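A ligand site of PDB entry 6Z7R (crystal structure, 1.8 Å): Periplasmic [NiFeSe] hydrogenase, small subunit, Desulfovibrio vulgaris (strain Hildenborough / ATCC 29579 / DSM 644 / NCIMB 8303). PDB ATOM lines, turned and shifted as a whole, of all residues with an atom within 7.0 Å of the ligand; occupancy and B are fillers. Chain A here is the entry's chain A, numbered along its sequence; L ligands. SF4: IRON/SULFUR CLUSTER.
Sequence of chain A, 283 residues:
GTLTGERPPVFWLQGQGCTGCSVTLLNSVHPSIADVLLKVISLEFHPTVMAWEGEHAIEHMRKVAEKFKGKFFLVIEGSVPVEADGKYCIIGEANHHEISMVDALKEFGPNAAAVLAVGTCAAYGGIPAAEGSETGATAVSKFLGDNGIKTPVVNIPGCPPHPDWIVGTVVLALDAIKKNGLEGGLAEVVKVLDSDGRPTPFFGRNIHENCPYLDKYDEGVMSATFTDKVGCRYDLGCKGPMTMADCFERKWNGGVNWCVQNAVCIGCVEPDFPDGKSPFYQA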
ATOM      1  N   ASN A 206       7.464  10.991  13.591  1.00  0.00           N
ATOM      2  CA  ASN A 206       6.943   9.659  13.327  1.00  0.00           C
ATOM      3  C   ASN A 206       6.023   9.210  14.464  1.00  0.00           C
ATOM      4  O   ASN A 206       6.253   9.539  15.630  1.00  0.00           O
ATOM      5  CB  ASN A 206       8.136   8.711  13.149  1.00  0.00           C
ATOM      6  CG  ASN A 206       7.738   7.270  13.096  1.00  0.00           C
ATOM      7  OD1 ASN A 206       7.584   6.637  14.126  1.00  0.00           O
ATOM      8  ND2 ASN A 206       7.654   6.702  11.897  1.00  0.00           N
ATOM      9  N   ILE A 207       4.920   8.538  14.114  1.00  0.00           N
ATOM     10  CA  ILE A 207       3.981   8.081  15.133  1.00  0.00           C
ATOM     11  C   ILE A 207       4.649   7.075  16.066  1.00  0.00           C
ATOM     12  O   ILE A 207       4.566   7.196  17.292  1.00  0.00           O
ATOM     13  CB  ILE A 207       2.712   7.461  14.514  1.00  0.00           C
ATOM     14  CG1 ILE A 207       1.879   8.513  13.804  1.00  0.00           C
ATOM     15  CG2 ILE A 207       1.877   6.749  15.588  1.00  0.00           C
ATOM     16  CD1 ILE A 207       0.942   9.309  14.773  1.00  0.00           C
ATOM     17  N   HIS A 208       5.223   6.016  15.478  1.00  0.00           N
ATOM     18  CA  HIS A 208       5.823   4.935  16.247  1.00  0.00           C
ATOM     19  C   HIS A 208       6.894   5.462  17.196  1.00  0.00           C
ATOM     20  O   HIS A 208       6.882   5.126  18.381  1.00  0.00           O
ATOM     21  CB  HIS A 208       6.392   3.896  15.280  1.00  0.00           C
ATOM     22  CG  HIS A 208       7.021   2.733  15.952  1.00  0.00           C
ATOM     23  ND1 HIS A 208       6.294   1.832  16.684  1.00  0.00           N
ATOM     24  CD2 HIS A 208       8.283   2.269  15.919  1.00  0.00           C
ATOM     25  CE1 HIS A 208       7.108   0.888  17.149  1.00  0.00           C
ATOM     26  NE2 HIS A 208       8.324   1.135  16.692  1.00  0.00           N
ATOM     27  N   GLU A 209       7.799   6.312  16.689  1.00  0.00           N
ATOM     28  CA  GLU A 209       8.861   6.844  17.537  1.00  0.00           C
ATOM     29  C   GLU A 209       8.300   7.518  18.779  1.00  0.00           C
ATOM     30  O   GLU A 209       9.004   7.640  19.781  1.00  0.00           O
ATOM     31  CB  GLU A 209       9.728   7.896  16.807  1.00  0.00           C
ATOM     32  CG  GLU A 209      10.830   7.361  15.877  1.00  0.00           C
ATOM     33  CD  GLU A 209      11.403   8.439  14.942  1.00  0.00           C
ATOM     34  OE1 GLU A 209      11.674   8.143  13.761  1.00  0.00           O
ATOM     35  OE2 GLU A 209      11.553   9.601  15.369  1.00  0.00           O
ATOM     36  N   ASN A 210       7.041   7.945  18.746  1.00  0.00           N
ATOM     37  CA  ASN A 210       6.487   8.692  19.867  1.00  0.00           C
ATOM     38  C   ASN A 210       5.272   8.023  20.492  1.00  0.00           C
ATOM     39  O   ASN A 210       4.553   8.673  21.247  1.00  0.00           O
ATOM     40  CB  ASN A 210       6.125  10.129  19.457  1.00  0.00           C
ATOM     41  CG  ASN A 210       7.346  10.989  19.201  1.00  0.00           C
ATOM     42  OD1 ASN A 210       7.859  11.667  20.117  1.00  0.00           O
ATOM     43  ND2 ASN A 210       7.832  10.984  17.945  1.00  0.00           N
ATOM     44  N   CYS A 211       5.040   6.684  20.212  1.00  0.00           N
ATOM     45  CA  CYS A 211       3.776   6.112  20.676  1.00  0.00           C
ATOM     46  C   CYS A 211       3.881   5.785  22.164  1.00  0.00           C
ATOM     47  O   CYS A 211       4.917   5.238  22.607  1.00  0.00           O
ATOM     48  CB  CYS A 211       3.392   4.841  19.872  1.00  0.00           C
ATOM     49  SG  CYS A 211       1.835   3.977  20.321  1.00  0.00           S
ATOM     50  N   PRO A 212       2.864   6.109  22.962  1.00  0.00           N
ATOM     51  CA  PRO A 212       2.892   5.739  24.388  1.00  0.00           C
ATOM     52  C   PRO A 212       2.955   4.226  24.621  1.00  0.00           C
ATOM     53  O   PRO A 212       3.256   3.773  25.724  1.00  0.00           O
ATOM     54  CB  PRO A 212       1.586   6.339  24.950  1.00  0.00           C
ATOM     55  CG  PRO A 212       0.704   6.545  23.799  1.00  0.00           C
ATOM     56  CD  PRO A 212       1.587   6.764  22.595  1.00  0.00           C
ATOM     57  N   TYR A 213       2.704   3.422  23.597  1.00  0.00           N
ATOM     58  CA  TYR A 213       2.838   1.983  23.732  1.00  0.00           C
ATOM     59  C   TYR A 213       4.179   1.521  23.209  1.00  0.00           C
ATOM     60  O   TYR A 213       4.387   0.324  23.001  1.00  0.00           O
ATOM     61  CB  TYR A 213       1.667   1.273  23.009  1.00  0.00           C
ATOM     62  CG  TYR A 213       0.336   1.854  23.465  1.00  0.00           C
ATOM     63  CD1 TYR A 213      -0.067   1.739  24.783  1.00  0.00           C
ATOM     64  CD2 TYR A 213      -0.514   2.503  22.586  1.00  0.00           C
ATOM     65  CE1 TYR A 213      -1.257   2.280  25.219  1.00  0.00           C
ATOM     66  CE2 TYR A 213      -1.699   3.025  23.032  1.00  0.00           C
ATOM     67  CZ  TYR A 213      -2.061   2.894  24.348  1.00  0.00           C
ATOM     68  OH  TYR A 213      -3.251   3.408  24.793  1.00  0.00           O
ATOM     69  N   LEU A 214       5.114   2.455  22.990  1.00  0.00           N
ATOM     70  CA  LEU A 214       6.407   2.048  22.478  1.00  0.00           C
ATOM     71  C   LEU A 214       7.100   1.132  23.482  1.00  0.00           C
ATOM     72  O   LEU A 214       7.831   0.214  23.096  1.00  0.00           O
ATOM     73  CB  LEU A 214       7.297   3.255  22.166  1.00  0.00           C
ATOM     74  CG  LEU A 214       8.564   2.947  21.313  1.00  0.00           C
ATOM     75  CD1 LEU A 214       8.270   2.168  19.996  1.00  0.00           C
ATOM     76  CD2 LEU A 214       9.347   4.221  21.028  1.00  0.00           C
ATOM     77  N   ASP A 215       6.855   1.343  24.790  1.00  0.00           N
ATOM     78  CA  ASP A 215       7.425   0.447  25.795  1.00  0.00           C
ATOM     79  C   ASP A 215       6.988  -0.989  25.525  1.00  0.00           C
ATOM     80  O   ASP A 215       7.820  -1.893  25.413  1.00  0.00           O
ATOM     81  CB  ASP A 215       6.970   0.863  27.201  1.00  0.00           C
ATOM     82  CG  ASP A 215       5.439   0.877  27.352  1.00  0.00           C
ATOM     83  OD1 ASP A 215       4.723   1.166  26.361  1.00  0.00           O
ATOM     84  OD2 ASP A 215       4.956   0.559  28.457  1.00  0.00           O
ATOM     85  N   LYS A 216       5.690  -1.182  25.267  1.00  0.00           N
ATOM     86  CA  LYS A 216       5.151  -2.507  25.026  1.00  0.00           C
ATOM     87  C   LYS A 216       5.655  -3.098  23.700  1.00  0.00           C
ATOM     88  O   LYS A 216       5.979  -4.285  23.635  1.00  0.00           O
ATOM     89  CB  LYS A 216       3.634  -2.406  25.031  1.00  0.00           C
ATOM     90  CG  LYS A 216       3.073  -1.760  26.281  1.00  0.00           C
ATOM     91  CD  LYS A 216       3.235  -2.686  27.443  1.00  0.00           C
ATOM     92  CE  LYS A 216       2.931  -1.991  28.740  1.00  0.00           C
ATOM     93  NZ  LYS A 216       3.129  -2.935  29.870  1.00  0.00           N
ATOM     94  N   TYR A 217       5.737  -2.298  22.640  1.00  0.00           N
ATOM     95  CA  TYR A 217       6.362  -2.786  21.418  1.00  0.00           C
ATOM     96  C   TYR A 217       7.727  -3.399  21.724  1.00  0.00           C
ATOM     97  O   TYR A 217       8.026  -4.519  21.290  1.00  0.00           O
ATOM     98  CB  TYR A 217       6.495  -1.640  20.414  1.00  0.00           C
ATOM     99  CG  TYR A 217       7.205  -2.012  19.134  1.00  0.00           C
ATOM    100  CD1 TYR A 217       6.491  -2.458  18.025  1.00  0.00           C
ATOM    101  CD2 TYR A 217       8.588  -1.921  19.016  1.00  0.00           C
ATOM    102  CE1 TYR A 217       7.128  -2.802  16.835  1.00  0.00           C
ATOM    103  CE2 TYR A 217       9.230  -2.260  17.843  1.00  0.00           C
ATOM    104  CZ  TYR A 217       8.486  -2.703  16.748  1.00  0.00           C
ATOM    105  OH  TYR A 217       9.106  -3.050  15.572  1.00  0.00           O
ATOM    106  N   ASP A 218       8.531  -2.677  22.506  1.00  0.00           N
ATOM    107  CA  ASP A 218       9.910  -3.088  22.748  1.00  0.00           C
ATOM    108  C   ASP A 218       9.939  -4.327  23.635  1.00  0.00           C
ATOM    109  O   ASP A 218      10.756  -5.224  23.429  1.00  0.00           O
ATOM    110  CB  ASP A 218      10.690  -1.949  23.397  1.00  0.00           C
ATOM    111  CG  ASP A 218      11.250  -0.965  22.375  1.00  0.00           C
ATOM    112  OD1 ASP A 218      11.570  -1.405  21.251  1.00  0.00           O
ATOM    113  OD2 ASP A 218      11.391   0.240  22.702  1.00  0.00           O
ATOM    114  N   MET A 222       2.052  -7.666  23.040  1.00  0.00           N
ATOM    115  CA  MET A 222       1.125  -7.335  21.959  1.00  0.00           C
ATOM    116  C   MET A 222      -0.316  -7.704  22.325  1.00  0.00           C
ATOM    117  O   MET A 222      -0.587  -8.838  22.742  1.00  0.00           O
ATOM    118  CB  MET A 222       1.516  -8.069  20.677  1.00  0.00           C
ATOM    119  CG  MET A 222       2.945  -7.819  20.219  1.00  0.00           C
ATOM    120  SD  MET A 222       3.178  -6.174  19.473  1.00  0.00           S
ATOM    121  CE  MET A 222       4.967  -6.199  19.202  1.00  0.00           C
ATOM    122  N   GLY A 231      -1.512  -3.804  25.609  1.00  0.00           N
ATOM    123  CA  GLY A 231      -0.401  -4.070  24.711  1.00  0.00           C
ATOM    124  C   GLY A 231      -0.293  -3.082  23.562  1.00  0.00           C
ATOM    125  O   GLY A 231      -1.152  -2.236  23.328  1.00  0.00           O
ATOM    126  N   CYS A 232       0.783  -3.256  22.791  1.00  0.00           N
ATOM    127  CA  CYS A 232       0.949  -2.563  21.529  1.00  0.00           C
ATOM    128  C   CYS A 232       0.005  -3.181  20.499  1.00  0.00           C
ATOM    129  O   CYS A 232      -0.297  -4.383  20.516  1.00  0.00           O
ATOM    130  CB  CYS A 232       2.421  -2.657  21.105  1.00  0.00           C
ATOM    131  SG  CYS A 232       2.873  -2.529  19.334  1.00  0.00           S
ATOM    132  N   ARG A 233      -0.480  -2.339  19.578  1.00  0.00           N
ATOM    133  CA  ARG A 233      -1.423  -2.748  18.550  1.00  0.00           C
ATOM    134  C   ARG A 233      -0.738  -3.282  17.299  1.00  0.00           C
ATOM    135  O   ARG A 233      -1.422  -3.560  16.322  1.00  0.00           O
ATOM    136  CB  ARG A 233      -2.299  -1.557  18.146  1.00  0.00           C
ATOM    137  CG  ARG A 233      -3.325  -1.138  19.145  1.00  0.00           C
ATOM    138  CD  ARG A 233      -2.776  -0.519  20.412  1.00  0.00           C
ATOM    139  NE  ARG A 233      -3.869   0.167  21.092  1.00  0.00           N
ATOM    140  CZ  ARG A 233      -3.946   0.415  22.391  1.00  0.00           C
ATOM    141  NH1 ARG A 233      -3.009   0.013  23.225  1.00  0.00           N
ATOM    142  NH2 ARG A 233      -5.002   1.052  22.866  1.00  0.00           N
ATOM    143  N   TYR A 234       0.578  -3.502  17.328  1.00  0.00           N
ATOM    144  CA  TYR A 234       1.315  -3.875  16.135  1.00  0.00           C
ATOM    145  C   TYR A 234       0.694  -5.090  15.453  1.00  0.00           C
ATOM    146  O   TYR A 234       0.409  -5.077  14.246  1.00  0.00           O
ATOM    147  CB  TYR A 234       2.780  -4.174  16.492  1.00  0.00           C
ATOM    148  CG  TYR A 234       3.584  -4.505  15.288  1.00  0.00           C
ATOM    149  CD1 TYR A 234       4.069  -3.505  14.464  1.00  0.00           C
ATOM    150  CD2 TYR A 234       3.857  -5.816  14.956  1.00  0.00           C
ATOM    151  CE1 TYR A 234       4.778  -3.797  13.317  1.00  0.00           C
ATOM    152  CE2 TYR A 234       4.573  -6.124  13.805  1.00  0.00           C
ATOM    153  CZ  TYR A 234       5.033  -5.111  12.998  1.00  0.00           C
ATOM    154  OH  TYR A 234       5.737  -5.411  11.849  1.00  0.00           O
ATOM    155  N   ASP A 235       0.473  -6.146  16.228  1.00  0.00           N
ATOM    156  CA  ASP A 235      -0.016  -7.382  15.632  1.00  0.00           C
ATOM    157  C   ASP A 235      -1.413  -7.212  15.053  1.00  0.00           C
ATOM    158  O   ASP A 235      -1.767  -7.944  14.122  1.00  0.00           O
ATOM    159  CB  ASP A 235      -0.030  -8.507  16.673  1.00  0.00           C
ATOM    160  CG  ASP A 235       1.357  -8.953  17.038  1.00  0.00           C
ATOM    161  OD1 ASP A 235       2.276  -8.778  16.180  1.00  0.00           O
ATOM    162  OD2 ASP A 235       1.493  -9.531  18.152  1.00  0.00           O
ATOM    163  N   GLY A 237      -2.290  -4.644  13.373  1.00  0.00           N
ATOM    164  CA  GLY A 237      -2.094  -3.980  12.090  1.00  0.00           C
ATOM    165  C   GLY A 237      -1.605  -2.531  12.162  1.00  0.00           C
ATOM    166  O   GLY A 237      -1.580  -1.838  11.142  1.00  0.00           O
ATOM    167  N   CYS A 238      -1.199  -2.063  13.333  1.00  0.00           N
ATOM    168  CA  CYS A 238      -0.839  -0.661  13.499  1.00  0.00           C
ATOM    169  C   CYS A 238       0.279  -0.251  12.532  1.00  0.00           C
ATOM    170  O   CYS A 238       1.290  -0.928  12.402  1.00  0.00           O
ATOM    171  CB  CYS A 238      -0.418  -0.400  14.930  1.00  0.00           C
ATOM    172  SG  CYS A 238      -0.281   1.357  15.270  1.00  0.00           S
ATOM    173  N   LYS A 239       0.079   0.871  11.847  1.00  0.00           N
ATOM    174  CA  LYS A 239       1.035   1.322  10.857  1.00  0.00           C
ATOM    175  C   LYS A 239       1.795   2.544  11.320  1.00  0.00           C
ATOM    176  O   LYS A 239       2.446   3.188  10.486  1.00  0.00           O
ATOM    177  CB  LYS A 239       0.331   1.599   9.523  1.00  0.00           C
ATOM    178  CG  LYS A 239      -0.427   0.386   8.968  1.00  0.00           C
ATOM    179  CD  LYS A 239       0.428  -0.874   8.995  1.00  0.00           C
ATOM    180  CE  LYS A 239      -0.203  -1.943   8.141  1.00  0.00           C
ATOM    181  NZ  LYS A 239      -1.571  -2.218   8.682  1.00  0.00           N
ATOM    182  N   GLY A 240       1.709   2.898  12.605  1.00  0.00           N
ATOM    183  CA  GLY A 240       2.582   3.876  13.206  1.00  0.00           C
ATOM    184  C   GLY A 240       4.022   3.796  12.711  1.00  0.00           C
ATOM    185  O   GLY A 240       4.608   4.799  12.310  1.00  0.00           O
ATOM    186  N   PRO A 241       4.622   2.610  12.683  1.00  0.00           N
ATOM    187  CA  PRO A 241       6.008   2.520  12.228  1.00  0.00           C
ATOM    188  C   PRO A 241       6.316   3.194  10.900  1.00  0.00           C
ATOM    189  O   PRO A 241       7.453   3.651  10.712  1.00  0.00           O
ATOM    190  CB  PRO A 241       6.233   0.988  12.136  1.00  0.00           C
ATOM    191  CG  PRO A 241       5.336   0.419  13.196  1.00  0.00           C
ATOM    192  CD  PRO A 241       4.099   1.309  13.172  1.00  0.00           C
ATOM    193  N   TRP A 258      -7.970   8.820  19.894  1.00  0.00           N
ATOM    194  CA  TRP A 258      -7.213   8.788  18.654  1.00  0.00           C
ATOM    195  C   TRP A 258      -7.089   7.351  18.188  1.00  0.00           C
ATOM    196  O   TRP A 258      -7.449   6.405  18.897  1.00  0.00           O
ATOM    197  CB  TRP A 258      -5.862   9.499  18.810  1.00  0.00           C
ATOM    198  CG  TRP A 258      -4.878   8.849  19.677  1.00  0.00           C
ATOM    199  CD1 TRP A 258      -5.013   8.610  21.012  1.00  0.00           C
ATOM    200  CD2 TRP A 258      -3.559   8.388  19.320  1.00  0.00           C
ATOM    201  NE1 TRP A 258      -3.879   8.002  21.487  1.00  0.00           N
ATOM    202  CE2 TRP A 258      -2.975   7.866  20.474  1.00  0.00           C
ATOM    203  CE3 TRP A 258      -2.821   8.374  18.112  1.00  0.00           C
ATOM    204  CZ2 TRP A 258      -1.678   7.334  20.477  1.00  0.00           C
ATOM    205  CZ3 TRP A 258      -1.552   7.848  18.116  1.00  0.00           C
ATOM    206  CH2 TRP A 258      -0.992   7.339  19.286  1.00  0.00           C
ATOM    207  N   VAL A 260      -4.699   5.041  17.394  1.00  0.00           N
ATOM    208  CA  VAL A 260      -3.937   4.009  18.120  1.00  0.00           C
ATOM    209  C   VAL A 260      -4.599   3.624  19.445  1.00  0.00           C
ATOM    210  O   VAL A 260      -4.551   2.459  19.863  1.00  0.00           O
ATOM    211  CB  VAL A 260      -2.477   4.443  18.356  1.00  0.00           C
ATOM    212  CG1 VAL A 260      -1.761   3.432  19.223  1.00  0.00           C
ATOM    213  CG2 VAL A 260      -1.710   4.525  17.075  1.00  0.00           C
ATOM    214  N   ALA A 263      -8.069   1.805  18.229  1.00  0.00           N
ATOM    215  CA  ALA A 263      -7.956   0.685  17.290  1.00  0.00           C
ATOM    216  C   ALA A 263      -6.536   0.541  16.759  1.00  0.00           C
ATOM    217  O   ALA A 263      -5.675  -0.040  17.428  1.00  0.00           O
ATOM    218  CB  ALA A 263      -8.947   0.879  16.133  1.00  0.00           C
ATOM    219  N   VAL A 264      -6.291   1.008  15.550  1.00  0.00           N
ATOM    220  CA  VAL A 264      -4.949   1.023  14.987  1.00  0.00           C
ATOM    221  C   VAL A 264      -4.780   2.306  14.181  1.00  0.00           C
ATOM    222  O   VAL A 264      -5.750   2.941  13.803  1.00  0.00           O
ATOM    223  CB  VAL A 264      -4.696  -0.187  14.082  1.00  0.00           C
ATOM    224  CG1 VAL A 264      -4.693  -1.482  14.913  1.00  0.00           C
ATOM    225  CG2 VAL A 264      -5.739  -0.252  12.976  1.00  0.00           C
ATOM    226  N   CYS A 265      -3.540   2.685  13.927  1.00  0.00           N
ATOM    227  CA  CYS A 265      -3.256   3.651  12.887  1.00  0.00           C
ATOM    228  C   CYS A 265      -3.279   2.944  11.529  1.00  0.00           C
ATOM    229  O   CYS A 265      -2.586   1.945  11.334  1.00  0.00           O
ATOM    230  CB  CYS A 265      -1.883   4.274  13.141  1.00  0.00           C
ATOM    231  SG  CYS A 265      -1.282   5.497  11.934  1.00  0.00           S
HETATM  232 FE1  SF4 L   1       1.573   1.164  16.710  1.00  0.00          FE
HETATM  233 FE2  SF4 L   1       4.227   1.505  17.101  1.00  0.00          FE
HETATM  234 FE3  SF4 L   1       2.802  -0.268  18.722  1.00  0.00          FE
HETATM  235 FE4  SF4 L   1       2.573   2.303  18.957  1.00  0.00          FE
HETATM  236  S1  SF4 L   1       4.510   1.158  19.357  1.00  0.00           S
HETATM  237  S2  SF4 L   1       0.774   0.870  18.819  1.00  0.00           S
HETATM  238  S3  SF4 L   1       2.660   3.170  16.775  1.00  0.00           S
HETATM  239  S4  SF4 L   1       3.221  -0.467  16.459  1.00  0.00           S
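A ring nitrogen (ND1) of His 208 is bound to an iron atom (FE2) of the ligand (2.1 Å). An iron atom (FE4) of the ligand is bound by the side-chain sulfur of Cys 211 (2.3 Å). An iron atom (FE3) of the ligand is bound by the side-chain sulfur (SG) of Cys 232 (2.3 Å). An iron atom (FE1) of the ligand is bound by the side-chain sulfur of Cys 238 (2.4 Å). S2 of the ligand lies close to N of Arg 233 (3.5 Å).
The backbone carbonyl oxygen (O) of Gly 240 lies within hydrogen-bond range of the backbone NH (N) of His 208 (3.4 Å). The side-chain sulfur (SG) of Cys 211 sits close to the backbone NH (N) of Tyr 213 (3.4 Å). The backbone carbonyl oxygen of Arg 233 lies within hydrogen-bond range of the backbone NH of Cys 238, at 3.4 Å. The side-chain sulfur of Cys 238 sits close to the backbone NH of Gly 240, at 3.7 Å. The backbone NH (N) of Cys 265 sits close to the side-chain sulfur (SG) of Cys 238 (3.8 Å). O of Val 260 sits at hydrogen-bond distance from NE of Arg 233 (2.7 Å). The guanidinium group of Arg 233 lies within hydrogen-bond range of the backbone carbonyl oxygen of Gly 231 (2.9 Å). The backbone carbonyl oxygen of Pro 241 lies within hydrogen-bond range of the side-chain amide nitrogen of Asn 206 (3.3 Å).
The backbone carbonyl oxygen (O) of Tyr 213 lies close to a sulfur (S1) of the ligand (3.7 Å). CG2 of Ile 207 touches S3 of the ligand, 3.9 Å away. Leu 214 touches the ligand (CA to S1, 3.8 Å). Tyr 217 touches the ligand. Tyr 234 touches the ligand. Gly 240 touches the ligand (CA to S3, 3.6 Å). Pro 241 touches the ligand. Val 260 touches the ligand (CG1 to S2, 3.6 Å). Hydrophobic or aromatic side chains within 4 Å of the ligand: Ile 207, His 208, Leu 214, Tyr 217, Tyr 234, Pro 241 and Val 260.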
